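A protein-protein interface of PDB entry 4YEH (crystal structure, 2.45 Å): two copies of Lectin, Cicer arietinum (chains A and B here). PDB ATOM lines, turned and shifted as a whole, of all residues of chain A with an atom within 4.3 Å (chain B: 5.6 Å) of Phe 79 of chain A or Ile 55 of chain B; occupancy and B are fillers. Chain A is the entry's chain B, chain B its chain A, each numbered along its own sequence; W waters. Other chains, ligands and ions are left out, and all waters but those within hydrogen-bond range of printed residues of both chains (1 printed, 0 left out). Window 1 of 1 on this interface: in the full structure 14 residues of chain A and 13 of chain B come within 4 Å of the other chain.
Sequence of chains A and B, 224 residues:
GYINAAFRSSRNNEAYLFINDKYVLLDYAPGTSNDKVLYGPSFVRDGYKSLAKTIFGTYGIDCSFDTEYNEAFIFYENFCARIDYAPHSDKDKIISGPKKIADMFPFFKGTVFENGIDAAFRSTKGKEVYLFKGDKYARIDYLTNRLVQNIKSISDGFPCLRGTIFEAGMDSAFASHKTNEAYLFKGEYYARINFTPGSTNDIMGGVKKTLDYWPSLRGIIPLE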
ATOM      1  N   ILE A  55       5.046 -16.761 -16.772  1.00  0.00           N
ATOM      2  CA  ILE A  55       3.821 -17.625 -16.679  1.00  0.00           C
ATOM      3  C   ILE A  55       2.870 -17.221 -15.533  1.00  0.00           C
ATOM      4  O   ILE A  55       1.633 -17.415 -15.599  1.00  0.00           O
ATOM      5  CB  ILE A  55       4.196 -19.092 -16.503  1.00  0.00           C
ATOM      6  CG1 ILE A  55       5.384 -19.179 -15.511  1.00  0.00           C
ATOM      7  CG2 ILE A  55       4.747 -19.611 -17.809  1.00  0.00           C
ATOM      8  CD1 ILE A  55       5.377 -20.267 -14.459  1.00  0.00           C
ATOM      9  N   PHE A  56       3.436 -16.641 -14.486  1.00  0.00           N
ATOM     10  CA  PHE A  56       2.610 -16.049 -13.445  1.00  0.00           C
ATOM     11  C   PHE A  56       1.804 -14.797 -13.919  1.00  0.00           C
ATOM     12  O   PHE A  56       0.603 -14.620 -13.530  1.00  0.00           O
ATOM     13  CB  PHE A  56       3.446 -15.753 -12.245  1.00  0.00           C
ATOM     14  CG  PHE A  56       4.307 -16.923 -11.789  1.00  0.00           C
ATOM     15  CD1 PHE A  56       3.757 -18.063 -11.248  1.00  0.00           C
ATOM     16  CD2 PHE A  56       5.662 -16.837 -11.851  1.00  0.00           C
ATOM     17  CE1 PHE A  56       4.547 -19.105 -10.855  1.00  0.00           C
ATOM     18  CE2 PHE A  56       6.494 -17.908 -11.445  1.00  0.00           C
ATOM     19  CZ  PHE A  56       5.930 -19.016 -10.941  1.00  0.00           C
ATOM     20  N   ILE A  74       5.679 -18.452  -4.643  1.00  0.00           N
ATOM     21  CA  ILE A  74       4.488 -18.481  -5.522  1.00  0.00           C
ATOM     22  C   ILE A  74       4.614 -19.576  -6.556  1.00  0.00           C
ATOM     23  O   ILE A  74       5.724 -19.848  -7.035  1.00  0.00           O
ATOM     24  CB  ILE A  74       4.269 -17.155  -6.328  1.00  0.00           C
ATOM     25  CG1 ILE A  74       5.477 -16.920  -7.231  1.00  0.00           C
ATOM     26  CG2 ILE A  74       3.928 -16.007  -5.380  1.00  0.00           C
ATOM     27  CD1 ILE A  74       5.493 -15.673  -8.062  1.00  0.00           C
ATOM     28  N   PHE A  75       3.480 -20.188  -6.882  1.00  0.00           N
ATOM     29  CA  PHE A  75       3.443 -21.404  -7.661  1.00  0.00           C
ATOM     30  C   PHE A  75       2.448 -21.304  -8.793  1.00  0.00           C
ATOM     31  O   PHE A  75       1.336 -20.720  -8.671  1.00  0.00           O
ATOM     32  CB  PHE A  75       3.044 -22.582  -6.797  1.00  0.00           C
ATOM     33  CG  PHE A  75       4.035 -22.884  -5.676  1.00  0.00           C
ATOM     34  CD1 PHE A  75       4.915 -23.947  -5.788  1.00  0.00           C
ATOM     35  CD2 PHE A  75       4.074 -22.091  -4.482  1.00  0.00           C
ATOM     36  CE1 PHE A  75       5.826 -24.230  -4.813  1.00  0.00           C
ATOM     37  CE2 PHE A  75       4.992 -22.384  -3.479  1.00  0.00           C
ATOM     38  CZ  PHE A  75       5.855 -23.457  -3.654  1.00  0.00           C
ATOM     39  N   TYR A  76       2.858 -21.891  -9.913  1.00  0.00           N
ATOM     40  CA  TYR A  76       1.908 -22.216 -10.985  1.00  0.00           C
ATOM     41  C   TYR A  76       2.344 -23.603 -11.559  1.00  0.00           C
ATOM     42  O   TYR A  76       3.451 -23.767 -12.052  1.00  0.00           O
ATOM     43  CB  TYR A  76       1.764 -21.071 -12.053  1.00  0.00           C
ATOM     44  CG  TYR A  76       0.784 -21.431 -13.120  1.00  0.00           C
ATOM     45  CD1 TYR A  76      -0.547 -21.393 -12.859  1.00  0.00           C
ATOM     46  CD2 TYR A  76       1.200 -21.875 -14.379  1.00  0.00           C
ATOM     47  CE1 TYR A  76      -1.494 -21.749 -13.815  1.00  0.00           C
ATOM     48  CE2 TYR A  76       0.291 -22.257 -15.344  1.00  0.00           C
ATOM     49  CZ  TYR A  76      -1.063 -22.180 -15.051  1.00  0.00           C
ATOM     50  OH  TYR A  76      -2.016 -22.544 -15.973  1.00  0.00           O
ATOM     51  N   GLU A  77       1.454 -24.598 -11.405  1.00  0.00           N
ATOM     52  CA  GLU A  77       1.690 -26.013 -11.794  1.00  0.00           C
ATOM     53  C   GLU A  77       3.038 -26.546 -11.328  1.00  0.00           C
ATOM     54  O   GLU A  77       3.250 -26.502 -10.115  1.00  0.00           O
ATOM     55  CB  GLU A  77       1.442 -26.224 -13.272  1.00  0.00           C
ATOM     56  CG  GLU A  77       0.124 -25.632 -13.693  1.00  0.00           C
ATOM     57  CD  GLU A  77      -0.165 -25.943 -15.127  1.00  0.00           C
ATOM     58  OE1 GLU A  77      -1.355 -26.047 -15.429  1.00  0.00           O
ATOM     59  OE2 GLU A  77       0.755 -26.078 -15.956  1.00  0.00           O
ATOM     60  N   ASN A  78       3.849 -27.137 -12.256  1.00  0.00           N
ATOM     61  CA  ASN A  78       5.282 -27.573 -12.080  1.00  0.00           C
ATOM     62  C   ASN A  78       6.195 -26.416 -11.536  1.00  0.00           C
ATOM     63  O   ASN A  78       7.301 -26.666 -11.050  1.00  0.00           O
ATOM     64  CB  ASN A  78       5.863 -27.907 -13.477  1.00  0.00           C
ATOM     65  CG  ASN A  78       5.940 -29.422 -13.826  1.00  0.00           C
ATOM     66  OD1 ASN A  78       6.224 -30.299 -12.990  1.00  0.00           O
ATOM     67  ND2 ASN A  78       5.763 -29.716 -15.115  1.00  0.00           N
ATOM     68  N   PHE A  79       5.741 -25.150 -11.655  1.00  0.00           N
ATOM     69  CA  PHE A  79       6.606 -23.965 -11.615  1.00  0.00           C
ATOM     70  C   PHE A  79       6.430 -22.981 -10.440  1.00  0.00           C
ATOM     71  O   PHE A  79       5.310 -22.683  -9.981  1.00  0.00           O
ATOM     72  CB  PHE A  79       6.521 -23.230 -12.951  1.00  0.00           C
ATOM     73  CG  PHE A  79       7.215 -23.951 -14.085  1.00  0.00           C
ATOM     74  CD1 PHE A  79       6.492 -24.660 -15.047  1.00  0.00           C
ATOM     75  CD2 PHE A  79       8.605 -23.939 -14.180  1.00  0.00           C
ATOM     76  CE1 PHE A  79       7.152 -25.346 -16.102  1.00  0.00           C
ATOM     77  CE2 PHE A  79       9.263 -24.606 -15.190  1.00  0.00           C
ATOM     78  CZ  PHE A  79       8.542 -25.324 -16.154  1.00  0.00           C
ATOM     79  N   CYS A  80       7.538 -22.500  -9.909  1.00  0.00           N
ATOM     80  CA  CYS A  80       7.462 -21.642  -8.762  1.00  0.00           C
ATOM     81  C   CYS A  80       8.575 -20.648  -8.757  1.00  0.00           C
ATOM     82  O   CYS A  80       9.510 -20.732  -9.512  1.00  0.00           O
ATOM     83  CB  CYS A  80       7.512 -22.466  -7.448  1.00  0.00           C
ATOM     84  SG  CYS A  80       9.014 -23.434  -7.181  1.00  0.00           S
ATOM     85  N   PRO A  98      11.902 -18.163 -12.283  1.00  0.00           N
ATOM     86  CA  PRO A  98      11.105 -19.363 -12.106  1.00  0.00           C
ATOM     87  C   PRO A  98      11.821 -20.677 -12.400  1.00  0.00           C
ATOM     88  O   PRO A  98      12.474 -20.818 -13.450  1.00  0.00           O
ATOM     89  CB  PRO A  98       9.946 -19.174 -13.086  1.00  0.00           C
ATOM     90  CG  PRO A  98      10.447 -18.200 -14.103  1.00  0.00           C
ATOM     91  CD  PRO A  98      11.394 -17.306 -13.380  1.00  0.00           C
ATOM     92  N   LYS A  99      11.655 -21.610 -11.444  1.00  0.00           N
ATOM     93  CA  LYS A  99      12.243 -22.962 -11.432  1.00  0.00           C
ATOM     94  C   LYS A  99      11.089 -23.948 -11.350  1.00  0.00           C
ATOM     95  O   LYS A  99      10.004 -23.588 -10.990  1.00  0.00           O
ATOM     96  CB  LYS A  99      13.077 -23.202 -10.165  1.00  0.00           C
ATOM     97  CG  LYS A  99      14.306 -22.363  -9.908  1.00  0.00           C
ATOM     98  CD  LYS A  99      14.975 -22.923  -8.635  1.00  0.00           C
ATOM     99  CE  LYS A  99      16.495 -22.740  -8.588  1.00  0.00           C
ATOM    100  NZ  LYS A  99      16.843 -21.323  -8.941  1.00  0.00           N
ATOM    101  N   LYS A 100      11.334 -25.197 -11.648  1.00  0.00           N
ATOM    102  CA  LYS A 100      10.372 -26.236 -11.403  1.00  0.00           C
ATOM    103  C   LYS A 100      10.232 -26.415  -9.880  1.00  0.00           C
ATOM    104  O   LYS A 100      11.035 -25.844  -9.131  1.00  0.00           O
ATOM    105  CB  LYS A 100      10.886 -27.499 -12.059  1.00  0.00           C
ATOM    106  CG  LYS A 100      10.786 -27.457 -13.564  1.00  0.00           C
ATOM    107  CD  LYS A 100      10.972 -28.833 -14.096  1.00  0.00           C
ATOM    108  CE  LYS A 100      10.709 -28.745 -15.558  1.00  0.00           C
ATOM    109  NZ  LYS A 100      11.728 -29.469 -16.336  1.00  0.00           N
ATOM    110  N   LEU B  51      14.584 -12.449 -21.366  1.00  0.00           N
ATOM    111  CA  LEU B  51      14.288 -13.834 -21.013  1.00  0.00           C
ATOM    112  C   LEU B  51      14.904 -14.240 -19.663  1.00  0.00           C
ATOM    113  O   LEU B  51      14.614 -15.321 -19.106  1.00  0.00           O
ATOM    114  CB  LEU B  51      14.759 -14.775 -22.135  1.00  0.00           C
ATOM    115  CG  LEU B  51      13.983 -14.961 -23.495  1.00  0.00           C
ATOM    116  CD1 LEU B  51      14.498 -16.163 -24.283  1.00  0.00           C
ATOM    117  CD2 LEU B  51      12.488 -15.099 -23.331  1.00  0.00           C
ATOM    118  N   LYS B  53      14.449 -13.484 -16.556  1.00  0.00           N
ATOM    119  CA  LYS B  53      13.620 -13.850 -15.458  1.00  0.00           C
ATOM    120  C   LYS B  53      12.495 -14.828 -15.765  1.00  0.00           C
ATOM    121  O   LYS B  53      11.489 -14.716 -15.218  1.00  0.00           O
ATOM    122  CB  LYS B  53      13.109 -12.613 -14.721  1.00  0.00           C
ATOM    123  CG  LYS B  53      14.105 -11.809 -13.937  1.00  0.00           C
ATOM    124  CD  LYS B  53      15.149 -12.578 -13.221  1.00  0.00           C
ATOM    125  CE  LYS B  53      14.606 -13.615 -12.295  1.00  0.00           C
ATOM    126  NZ  LYS B  53      15.630 -14.090 -11.321  1.00  0.00           N
ATOM    127  N   THR B  54      12.679 -15.732 -16.705  1.00  0.00           N
ATOM    128  CA  THR B  54      11.676 -16.644 -17.256  1.00  0.00           C
ATOM    129  C   THR B  54      12.130 -18.108 -17.191  1.00  0.00           C
ATOM    130  O   THR B  54      13.283 -18.407 -16.966  1.00  0.00           O
ATOM    131  CB  THR B  54      11.212 -16.312 -18.733  1.00  0.00           C
ATOM    132  OG1 THR B  54      12.295 -16.467 -19.691  1.00  0.00           O
ATOM    133  CG2 THR B  54      10.623 -14.915 -18.837  1.00  0.00           C
ATOM    134  N   ILE B  55      11.188 -19.020 -17.403  1.00  0.00           N
ATOM    135  CA  ILE B  55      11.467 -20.435 -17.489  1.00  0.00           C
ATOM    136  C   ILE B  55      12.477 -20.752 -18.603  1.00  0.00           C
ATOM    137  O   ILE B  55      13.261 -21.676 -18.477  1.00  0.00           O
ATOM    138  CB  ILE B  55      10.165 -21.229 -17.700  1.00  0.00           C
ATOM    139  CG1 ILE B  55       9.432 -20.689 -18.941  1.00  0.00           C
ATOM    140  CG2 ILE B  55       9.288 -21.136 -16.444  1.00  0.00           C
ATOM    141  CD1 ILE B  55       8.374 -21.589 -19.559  1.00  0.00           C
ATOM    142  N   PHE B  56      12.477 -19.964 -19.678  1.00  0.00           N
ATOM    143  CA  PHE B  56      13.443 -20.093 -20.749  1.00  0.00           C
ATOM    144  C   PHE B  56      14.894 -19.736 -20.320  1.00  0.00           C
ATOM    145  O   PHE B  56      15.831 -20.401 -20.742  1.00  0.00           O
ATOM    146  CB  PHE B  56      13.044 -19.180 -21.936  1.00  0.00           C
ATOM    147  CG  PHE B  56      11.657 -19.436 -22.482  1.00  0.00           C
ATOM    148  CD1 PHE B  56      11.328 -20.660 -23.086  1.00  0.00           C
ATOM    149  CD2 PHE B  56      10.667 -18.468 -22.415  1.00  0.00           C
ATOM    150  CE1 PHE B  56      10.057 -20.871 -23.585  1.00  0.00           C
ATOM    151  CE2 PHE B  56       9.387 -18.710 -22.889  1.00  0.00           C
ATOM    152  CZ  PHE B  56       9.088 -19.902 -23.472  1.00  0.00           C
ATOM    153  N   GLY B  57      15.062 -18.692 -19.495  1.00  0.00           N
ATOM    154  CA  GLY B  57      16.351 -18.266 -18.972  1.00  0.00           C
ATOM    155  C   GLY B  57      16.829 -19.328 -18.019  1.00  0.00           C
ATOM    156  O   GLY B  57      18.038 -19.672 -18.011  1.00  0.00           O
ATOM    157  N   THR B  58      15.907 -19.845 -17.185  1.00  0.00           N
ATOM    158  CA  THR B  58      16.263 -20.981 -16.292  1.00  0.00           C
ATOM    159  C   THR B  58      16.666 -22.295 -17.011  1.00  0.00           C
ATOM    160  O   THR B  58      17.601 -22.962 -16.548  1.00  0.00           O
ATOM    161  CB  THR B  58      15.139 -21.259 -15.260  1.00  0.00           C
ATOM    162  OG1 THR B  58      14.704 -20.009 -14.699  1.00  0.00           O
ATOM    163  CG2 THR B  58      15.599 -22.152 -14.174  1.00  0.00           C
ATOM    164  N   TYR B  59      15.884 -22.699 -18.010  1.00  0.00           N
ATOM    165  CA  TYR B  59      16.040 -24.017 -18.611  1.00  0.00           C
ATOM    166  C   TYR B  59      16.450 -24.067 -20.082  1.00  0.00           C
ATOM    167  O   TYR B  59      16.668 -25.157 -20.613  1.00  0.00           O
ATOM    168  CB  TYR B  59      14.762 -24.840 -18.409  1.00  0.00           C
ATOM    169  CG  TYR B  59      14.471 -25.172 -16.962  1.00  0.00           C
ATOM    170  CD1 TYR B  59      15.230 -26.112 -16.280  1.00  0.00           C
ATOM    171  CD2 TYR B  59      13.437 -24.544 -16.281  1.00  0.00           C
ATOM    172  CE1 TYR B  59      14.967 -26.419 -14.957  1.00  0.00           C
ATOM    173  CE2 TYR B  59      13.167 -24.845 -14.959  1.00  0.00           C
ATOM    174  CZ  TYR B  59      13.934 -25.782 -14.303  1.00  0.00           C
ATOM    175  OH  TYR B  59      13.669 -26.085 -12.987  1.00  0.00           O
ATOM    176  N   GLY B  60      16.561 -22.925 -20.755  1.00  0.00           N
ATOM    177  CA  GLY B  60      16.936 -22.996 -22.152  1.00  0.00           C
ATOM    178  C   GLY B  60      15.706 -23.136 -23.016  1.00  0.00           C
ATOM    179  O   GLY B  60      14.569 -23.058 -22.520  1.00  0.00           O
ATOM    180  N   TYR B  76       9.462 -24.207 -24.500  1.00  0.00           N
ATOM    181  CA  TYR B  76      10.073 -25.112 -23.527  1.00  0.00           C
ATOM    182  C   TYR B  76       8.922 -25.832 -22.851  1.00  0.00           C
ATOM    183  O   TYR B  76       8.105 -25.170 -22.214  1.00  0.00           O
ATOM    184  CB  TYR B  76      10.879 -24.363 -22.458  1.00  0.00           C
ATOM    185  CG  TYR B  76      11.362 -25.296 -21.420  1.00  0.00           C
ATOM    186  CD1 TYR B  76      12.464 -26.095 -21.651  1.00  0.00           C
ATOM    187  CD2 TYR B  76      10.672 -25.458 -20.235  1.00  0.00           C
ATOM    188  CE1 TYR B  76      12.908 -26.992 -20.701  1.00  0.00           C
ATOM    189  CE2 TYR B  76      11.108 -26.352 -19.267  1.00  0.00           C
ATOM    190  CZ  TYR B  76      12.219 -27.134 -19.524  1.00  0.00           C
ATOM    191  OH  TYR B  76      12.663 -28.044 -18.588  1.00  0.00           O
ATOM    192  N   GLU B  77       8.856 -27.165 -23.026  1.00  0.00           N
ATOM    193  CA  GLU B  77       7.734 -27.991 -22.582  1.00  0.00           C
ATOM    194  C   GLU B  77       6.426 -27.370 -23.068  1.00  0.00           C
ATOM    195  O   GLU B  77       6.366 -26.924 -24.212  1.00  0.00           O
ATOM    196  CB  GLU B  77       7.752 -28.198 -21.065  1.00  0.00           C
ATOM    197  CG  GLU B  77       8.783 -29.209 -20.637  1.00  0.00           C
ATOM    198  CD  GLU B  77       9.011 -29.251 -19.138  1.00  0.00           C
ATOM    199  OE1 GLU B  77       8.095 -28.940 -18.360  1.00  0.00           O
ATOM    200  OE2 GLU B  77      10.133 -29.619 -18.740  1.00  0.00           O
ATOM    201  N   PHE B  79       4.976 -24.612 -22.780  1.00  0.00           N
ATOM    202  CA  PHE B  79       4.902 -23.136 -22.842  1.00  0.00           C
ATOM    203  C   PHE B  79       5.693 -22.665 -24.008  1.00  0.00           C
ATOM    204  O   PHE B  79       6.544 -23.425 -24.528  1.00  0.00           O
ATOM    205  CB  PHE B  79       5.439 -22.449 -21.572  1.00  0.00           C
ATOM    206  CG  PHE B  79       4.655 -22.762 -20.344  1.00  0.00           C
ATOM    207  CD1 PHE B  79       5.155 -23.670 -19.420  1.00  0.00           C
ATOM    208  CD2 PHE B  79       3.356 -22.248 -20.150  1.00  0.00           C
ATOM    209  CE1 PHE B  79       4.410 -24.016 -18.296  1.00  0.00           C
ATOM    210  CE2 PHE B  79       2.628 -22.593 -19.014  1.00  0.00           C
ATOM    211  CZ  PHE B  79       3.171 -23.480 -18.089  1.00  0.00           C
ATOM    212  N   PRO B  98       4.633 -15.292 -22.207  1.00  0.00           N
ATOM    213  CA  PRO B  98       4.544 -16.768 -22.414  1.00  0.00           C
ATOM    214  C   PRO B  98       3.176 -17.439 -22.170  1.00  0.00           C
ATOM    215  O   PRO B  98       2.657 -17.393 -21.090  1.00  0.00           O
ATOM    216  CB  PRO B  98       5.552 -17.321 -21.417  1.00  0.00           C
ATOM    217  CG  PRO B  98       5.394 -16.342 -20.247  1.00  0.00           C
ATOM    218  CD  PRO B  98       5.225 -14.954 -20.891  1.00  0.00           C
HETATM  219  O   HOH W   1       8.142 -17.538 -16.961  1.00  0.00           O
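The backbone carbonyl oxygen of Pro 98 of chain A sits at hydrogen-bond distance from the side-chain hydroxyl of Thr 58 of chain B, at 2.7 Å. N of Lys 100 of chain A is in hydrogen-bond range of OH of Tyr 59 of chain B (2.8 Å). The side-chain amino group of Lys 100 of chain A sits at hydrogen-bond distance from the side-chain hydroxyl of Tyr 76 of chain B, 2.8 Å away. The side-chain carboxylate of Glu 77 of chain B is in salt-bridge range of the side-chain amino group of Lys 100 of chain A, at 2.9 Å.
The backbone carbonyl oxygen (O) of Leu 51 of chain B lies within hydrogen-bond range of the side-chain hydroxyl (OG1) of Thr 54 of chain B (2.7 Å). The side-chain hydroxyl (OG1) of Thr 58 of chain B lies within hydrogen-bond range of the backbone carbonyl oxygen (O) of Thr 54 of chain B, 3.1 Å away. The side-chain hydroxyl (OH) of Tyr 76 of chain B is in hydrogen-bond range of the side-chain carboxylate (OE2) of Glu 77 of chain B. The backbone NH (N) of Cys 80 of chain A lies within hydrogen-bond range of the backbone carbonyl oxygen (O) of Lys 99 of chain A (2.9 Å). The side-chain sulfur (SG) of Cys 80 of chain A sits at hydrogen-bond distance from the backbone carbonyl oxygen (O) of Lys 100 of chain A (3.7 Å).
Phe 79 of chain B touches Ile 55 of chain A. Ile 55 of chain A touches Pro 98 of chain B (N to CG, 3.5 Å). Ile 55 of chain B touches Phe 79 of chain A. CE2 of Phe 79 of chain A touches CE2 of Tyr 59 of chain B, at 3.9 Å. CE1 of Phe 79 of chain B touches CE1 of Phe 79 of chain A, at 3.8 Å. Pro 98 of chain A touches Lys 53 of chain B (CD to O, 3.2 Å). Thr 54 of chain B touches Pro 98 of chain A (C to CG, 3.5 Å). Pro 98 of chain A touches Ile 55 of chain B (CG to N, 3.5 Å). Lys 99 of chain A touches Tyr 59 of chain B (C to OH, 3.7 Å).
Phe 79 of chain A touches three residues of chain B. Of chain A, only Phe 79 (3.7 Å) and Pro 98 (3.5 Å) come within 4 Å of Ile 55 of chain B. Printed residues of chain A within 4 Å of Lys 53 of chain B: Pro 98 (3.2 Å). Printed residues of chain A within 4 Å of Tyr 76 of chain B: Lys 100 (2.8 Å). Asn 78 of chain A touches none of the printed residues of chain B. The nearest residue of chain B that does not touch Phe 79 of chain A is Tyr 76 of chain B (4.2 Å). The nearest printed residue of chain A that does not touch Ile 55 of chain B is Ile 55 of chain A (4.5 Å). The nearest printed residue of chain B that does not touch Pro 98 of chain A is Tyr 59 of chain B (4.4 Å).
Of the 12 printed residues of chain A, 5 touch a printed residue of chain B. Among the printed residues, 13 pairs touch across the chains. Among the printed residues, Asp or Glu carboxylates within 4 Å of a Lys or Arg side-chain nitrogen of the other chain: Lys 100 of chain A with Glu 77 of chain B (2.9 Å).
Ile 55 of chain A touches Phe 79 of chain B, and with the chains exchanged Phe 79 of chain A touches Ile 55 of chain B. Ile 55 of chain A touches Pro 98 of chain B, and with the chains exchanged Pro 98 of chain A touches Ile 55 of chain B. Phe 79 of chain A touches its own counterpart, Phe 79 of chain B.
Water W1 lies within hydrogen-bond range of N of Ile 55 of chain A and N of Ile 55 of chain B.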
